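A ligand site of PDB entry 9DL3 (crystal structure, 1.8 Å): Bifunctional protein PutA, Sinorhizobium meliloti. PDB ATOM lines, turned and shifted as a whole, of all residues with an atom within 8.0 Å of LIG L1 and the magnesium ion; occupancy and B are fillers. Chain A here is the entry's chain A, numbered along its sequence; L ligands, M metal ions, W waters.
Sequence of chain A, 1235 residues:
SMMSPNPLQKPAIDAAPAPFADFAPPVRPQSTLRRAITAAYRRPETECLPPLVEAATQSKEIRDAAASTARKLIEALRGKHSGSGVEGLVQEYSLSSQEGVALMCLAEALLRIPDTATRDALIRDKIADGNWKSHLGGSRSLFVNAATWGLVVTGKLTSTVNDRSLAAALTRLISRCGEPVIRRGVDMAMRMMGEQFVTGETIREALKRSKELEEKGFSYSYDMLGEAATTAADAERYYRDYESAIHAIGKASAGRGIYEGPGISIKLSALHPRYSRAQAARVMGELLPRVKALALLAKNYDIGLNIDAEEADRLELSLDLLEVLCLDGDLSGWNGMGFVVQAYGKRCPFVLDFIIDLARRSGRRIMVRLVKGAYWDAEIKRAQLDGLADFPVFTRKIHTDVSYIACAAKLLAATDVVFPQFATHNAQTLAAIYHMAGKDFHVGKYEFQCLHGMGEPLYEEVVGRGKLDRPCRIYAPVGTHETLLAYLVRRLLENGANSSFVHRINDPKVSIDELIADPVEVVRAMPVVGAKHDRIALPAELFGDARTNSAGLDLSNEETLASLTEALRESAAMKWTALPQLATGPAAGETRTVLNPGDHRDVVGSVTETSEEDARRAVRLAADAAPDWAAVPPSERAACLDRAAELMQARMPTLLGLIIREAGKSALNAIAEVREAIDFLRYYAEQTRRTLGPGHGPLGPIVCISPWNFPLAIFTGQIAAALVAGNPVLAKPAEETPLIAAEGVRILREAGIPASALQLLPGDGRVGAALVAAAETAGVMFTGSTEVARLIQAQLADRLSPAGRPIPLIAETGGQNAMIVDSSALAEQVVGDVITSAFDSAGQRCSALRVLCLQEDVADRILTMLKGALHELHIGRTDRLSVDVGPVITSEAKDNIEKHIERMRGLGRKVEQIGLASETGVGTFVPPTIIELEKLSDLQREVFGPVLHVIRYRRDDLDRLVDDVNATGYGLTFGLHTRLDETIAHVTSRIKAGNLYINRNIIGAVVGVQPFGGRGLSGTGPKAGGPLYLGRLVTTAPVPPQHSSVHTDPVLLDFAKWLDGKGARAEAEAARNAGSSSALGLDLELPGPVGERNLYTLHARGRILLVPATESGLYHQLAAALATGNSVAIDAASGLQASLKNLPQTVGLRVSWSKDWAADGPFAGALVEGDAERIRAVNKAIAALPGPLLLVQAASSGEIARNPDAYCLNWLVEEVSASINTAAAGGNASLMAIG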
ATOM      1  N   GLU A 612       7.051  -7.744  -4.869  1.00  0.00           N
ATOM      2  CA  GLU A 612       6.742  -7.452  -3.475  1.00  0.00           C
ATOM      3  C   GLU A 612       7.421  -8.452  -2.540  1.00  0.00           C
ATOM      4  O   GLU A 612       7.871  -8.079  -1.455  1.00  0.00           O
ATOM      5  CB  GLU A 612       5.226  -7.422  -3.254  1.00  0.00           C
ATOM      6  CG  GLU A 612       4.587  -6.158  -3.796  1.00  0.00           C
ATOM      7  CD  GLU A 612       3.092  -6.093  -3.554  1.00  0.00           C
ATOM      8  OE1 GLU A 612       2.639  -6.528  -2.468  1.00  0.00           O
ATOM      9  OE2 GLU A 612       2.368  -5.617  -4.457  1.00  0.00           O
ATOM     10  N   GLU A 735       9.579   5.396  -9.960  1.00  0.00           N
ATOM     11  CA  GLU A 735       9.516   4.421 -11.046  1.00  0.00           C
ATOM     12  C   GLU A 735       9.944   5.030 -12.371  1.00  0.00           C
ATOM     13  O   GLU A 735      10.426   4.311 -13.256  1.00  0.00           O
ATOM     14  CB  GLU A 735       8.106   3.834 -11.172  1.00  0.00           C
ATOM     15  CG  GLU A 735       7.088   4.802 -11.697  1.00  0.00           C
ATOM     16  CD  GLU A 735       5.700   4.450 -11.206  1.00  0.00           C
ATOM     17  OE1 GLU A 735       5.457   4.519  -9.974  1.00  0.00           O
ATOM     18  OE2 GLU A 735       4.859   4.097 -12.044  1.00  0.00           O
ATOM     19  N   GLU A 736       9.812   6.351 -12.519  1.00  0.00           N
ATOM     20  CA  GLU A 736      10.194   6.999 -13.770  1.00  0.00           C
ATOM     21  C   GLU A 736      11.698   7.120 -13.953  1.00  0.00           C
ATOM     22  O   GLU A 736      12.165   7.224 -15.094  1.00  0.00           O
ATOM     23  CB  GLU A 736       9.568   8.401 -13.864  1.00  0.00           C
ATOM     24  CG  GLU A 736       8.031   8.423 -13.828  1.00  0.00           C
ATOM     25  CD  GLU A 736       7.446   8.412 -12.416  1.00  0.00           C
ATOM     26  OE1 GLU A 736       8.196   8.213 -11.431  1.00  0.00           O
ATOM     27  OE2 GLU A 736       6.212   8.624 -12.292  1.00  0.00           O
ATOM     28  N   GLY A 763      10.839   0.055  -8.776  1.00  0.00           N
ATOM     29  CA  GLY A 763       9.490  -0.386  -9.112  1.00  0.00           C
ATOM     30  C   GLY A 763       8.463   0.706  -8.877  1.00  0.00           C
ATOM     31  O   GLY A 763       8.809   1.879  -8.724  1.00  0.00           O
ATOM     32  N   ASP A 764       7.190   0.295  -8.870  1.00  0.00           N
ATOM     33  CA  ASP A 764       6.074   1.224  -8.776  1.00  0.00           C
ATOM     34  C   ASP A 764       5.665   1.402  -7.314  1.00  0.00           C
ATOM     35  O   ASP A 764       6.356   0.966  -6.388  1.00  0.00           O
ATOM     36  CB  ASP A 764       4.923   0.756  -9.668  1.00  0.00           C
ATOM     37  CG  ASP A 764       4.446  -0.668  -9.353  1.00  0.00           C
ATOM     38  OD1 ASP A 764       4.675  -1.166  -8.225  1.00  0.00           O
ATOM     39  OD2 ASP A 764       3.824  -1.289 -10.248  1.00  0.00           O
ATOM     40  N   GLY A 765       4.521   2.053  -7.085  1.00  0.00           N
ATOM     41  CA  GLY A 765       4.106   2.387  -5.720  1.00  0.00           C
ATOM     42  C   GLY A 765       3.873   1.177  -4.832  1.00  0.00           C
ATOM     43  O   GLY A 765       3.965   1.277  -3.605  1.00  0.00           O
ATOM     44  N   ARG A 766       3.556   0.024  -5.433  1.00  0.00           N
ATOM     45  CA  ARG A 766       3.314  -1.177  -4.654  1.00  0.00           C
ATOM     46  C   ARG A 766       4.586  -1.656  -3.979  1.00  0.00           C
ATOM     47  O   ARG A 766       4.548  -2.177  -2.865  1.00  0.00           O
ATOM     48  CB  ARG A 766       2.726  -2.289  -5.533  1.00  0.00           C
ATOM     49  N   VAL A 767       5.733  -1.499  -4.650  1.00  0.00           N
ATOM     50  CA  VAL A 767       7.024  -1.795  -4.050  1.00  0.00           C
ATOM     51  C   VAL A 767       7.271  -0.894  -2.840  1.00  0.00           C
ATOM     52  O   VAL A 767       7.621  -1.371  -1.749  1.00  0.00           O
ATOM     53  CB  VAL A 767       8.153  -1.641  -5.079  1.00  0.00           C
ATOM     54  CG1 VAL A 767       9.520  -1.831  -4.398  1.00  0.00           C
ATOM     55  CG2 VAL A 767       7.949  -2.610  -6.235  1.00  0.00           C
ATOM     56  N   GLY A 768       7.076   0.407  -3.012  1.00  0.00           N
ATOM     57  CA  GLY A 768       7.253   1.330  -1.903  1.00  0.00           C
ATOM     58  C   GLY A 768       6.316   1.039  -0.750  1.00  0.00           C
ATOM     59  O   GLY A 768       6.700   1.147   0.413  1.00  0.00           O
ATOM     60  N   ALA A 769       5.073   0.661  -1.042  1.00  0.00           N
ATOM     61  CA  ALA A 769       4.128   0.339   0.016  1.00  0.00           C
ATOM     62  C   ALA A 769       4.565  -0.901   0.774  1.00  0.00           C
ATOM     63  O   ALA A 769       4.415  -0.986   2.004  1.00  0.00           O
ATOM     64  CB  ALA A 769       2.721   0.123  -0.571  1.00  0.00           C
ATOM     65  N   SER A 785       4.677  13.450  -3.599  1.00  0.00           N
ATOM     66  CA  SER A 785       3.350  14.040  -3.575  1.00  0.00           C
ATOM     67  C   SER A 785       2.730  13.968  -2.177  1.00  0.00           C
ATOM     68  O   SER A 785       3.004  13.064  -1.393  1.00  0.00           O
ATOM     69  CB  SER A 785       2.430  13.349  -4.567  1.00  0.00           C
ATOM     70  OG  SER A 785       2.138  12.021  -4.154  1.00  0.00           O
ATOM     71  N   GLU A 787      -0.309  13.160  -1.674  1.00  0.00           N
ATOM     72  CA  GLU A 787      -1.123  11.958  -1.690  1.00  0.00           C
ATOM     73  C   GLU A 787      -0.356  10.748  -1.160  1.00  0.00           C
ATOM     74  O   GLU A 787      -0.833  10.021  -0.282  1.00  0.00           O
ATOM     75  CB  GLU A 787      -1.621  11.702  -3.102  1.00  0.00           C
ATOM     76  CG  GLU A 787      -2.074  10.284  -3.354  1.00  0.00           C
ATOM     77  CD  GLU A 787      -2.221   9.978  -4.837  1.00  0.00           C
ATOM     78  OE1 GLU A 787      -1.790  10.808  -5.682  1.00  0.00           O
ATOM     79  OE2 GLU A 787      -2.774   8.905  -5.142  1.00  0.00           O
ATOM     80  N   VAL A 788       0.848  10.513  -1.694  1.00  0.00           N
ATOM     81  CA  VAL A 788       1.606   9.352  -1.244  1.00  0.00           C
ATOM     82  C   VAL A 788       2.104   9.569   0.184  1.00  0.00           C
ATOM     83  O   VAL A 788       2.139   8.629   0.984  1.00  0.00           O
ATOM     84  CB  VAL A 788       2.754   9.055  -2.221  1.00  0.00           C
ATOM     85  CG1 VAL A 788       3.655   7.963  -1.636  1.00  0.00           C
ATOM     86  CG2 VAL A 788       2.187   8.595  -3.563  1.00  0.00           C
ATOM     87  N   LEU A 791      -0.620   8.468   2.438  1.00  0.00           N
ATOM     88  CA  LEU A 791      -0.707   7.013   2.471  1.00  0.00           C
ATOM     89  C   LEU A 791       0.384   6.402   3.332  1.00  0.00           C
ATOM     90  O   LEU A 791       0.150   5.431   4.059  1.00  0.00           O
ATOM     91  CB  LEU A 791      -0.607   6.442   1.062  1.00  0.00           C
ATOM     92  CG  LEU A 791      -1.731   6.811   0.100  1.00  0.00           C
ATOM     93  CD1 LEU A 791      -1.424   6.245  -1.283  1.00  0.00           C
ATOM     94  CD2 LEU A 791      -3.048   6.278   0.637  1.00  0.00           C
HETATM   95  C1  LIG L   1       1.377   1.099  -8.020  1.00  0.00           C
HETATM   96  O1  LIG L   1       1.551  -0.075  -7.651  1.00  0.00           O
HETATM   97  N1  LIG L   1       0.579   3.282  -7.356  1.00  0.00           N
HETATM   98  C2  LIG L   1       0.662   2.018  -7.033  1.00  0.00           C
HETATM   99  C3  LIG L   1       0.125   1.501  -5.825  1.00  0.00           C
HETATM  100  C4  LIG L   1      -0.515   2.341  -4.973  1.00  0.00           C
HETATM  101  C5  LIG L   1      -1.268   4.648  -4.468  1.00  0.00           C
HETATM  102  C6  LIG L   1      -1.326   5.962  -4.840  1.00  0.00           C
HETATM  103  C7  LIG L   1      -0.747   6.391  -6.061  1.00  0.00           C
HETATM  104  C8  LIG L   1      -0.117   5.499  -6.892  1.00  0.00           C
HETATM  105  C9  LIG L   1      -0.616   3.710  -5.293  1.00  0.00           C
HETATM  106  C10 LIG L   1      -0.046   4.135  -6.520  1.00  0.00           C
HETATM  107  O2  LIG L   1       1.703   1.638  -9.085  1.00  0.00           O
HETATM  108  C1  LG2 L   2       6.581   5.462  -4.934  1.00  0.00           C
HETATM  109  O1  LG2 L   2       6.017   5.980  -5.921  1.00  0.00           O
HETATM  110  N1  LG2 L   2       4.448   5.036  -3.790  1.00  0.00           N
HETATM  111  C2  LG2 L   2       5.736   5.060  -3.706  1.00  0.00           C
HETATM  112  C3  LG2 L   2       6.408   4.733  -2.500  1.00  0.00           C
HETATM  113  C4  LG2 L   2       5.718   4.365  -1.383  1.00  0.00           C
HETATM  114  C5  LG2 L   2       3.520   3.947  -0.358  1.00  0.00           C
HETATM  115  C6  LG2 L   2       2.156   3.921  -0.508  1.00  0.00           C
HETATM  116  C7  LG2 L   2       1.567   4.267  -1.750  1.00  0.00           C
HETATM  117  C8  LG2 L   2       2.327   4.628  -2.825  1.00  0.00           C
HETATM  118  C9  LG2 L   2       4.320   4.327  -1.459  1.00  0.00           C
HETATM  119  C10 LG2 L   2       3.727   4.660  -2.702  1.00  0.00           C
HETATM  120  O2  LG2 L   2       7.786   5.201  -4.815  1.00  0.00           O
HETATM  121 MG    MG M   1       1.390   3.651  -9.470  1.00  0.00          MG
HETATM  122  O   HOH W   1       1.273  -2.311  -9.119  1.00  0.00           O
HETATM  123  O   HOH W   2       3.216   4.064  -8.577  1.00  0.00           O
HETATM  124  O   HOH W   3       2.497   3.232 -11.213  1.00  0.00           O
HETATM  125  O   HOH W   4       1.073   5.715  -9.827  1.00  0.00           O
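OD1 of Asp 764 sits close to O1 of LIG L1 (3.4 Å).
Residues that only touch LIG L1: Glu 787 and Leu 791.
Hydrophobic or aromatic side chains that line LIG L1: Leu 791.
The nearest printed residue that does not touch LIG L1 is Val 788 (4.4 Å).
No residue comes within 4 Å of the magnesium ion.
Water W2 lies within hydrogen-bond range of OE1 of Glu 735 (2.7 Å) and N of Gly 765 (2.8 Å).
Water W1 bridges O1 of LIG L1 (2.7 Å) and OD2 of Asp 764 (3.0 Å).
N of Arg 766 lies close to OD1 of Asp 764 (3.2 Å).
O1 of LIG L1 lies within hydrogen-bond range of N of Arg 766, 3.0 Å away.
An oxygen (O2) of LIG L1 sits close to the backbone NH of Gly 765 (3.5 Å).
O2 of LIG L1 is bound to the magnesium ion (2.1 Å).
The magnesium ion is bound by water W2, 2.1 Å away.
Water W3 is bound to the magnesium ion (2.1 Å).
The magnesium ion is bound by water W4 (2.1 Å).
N1 of LIG L1 binds the magnesium ion (2.3 Å).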
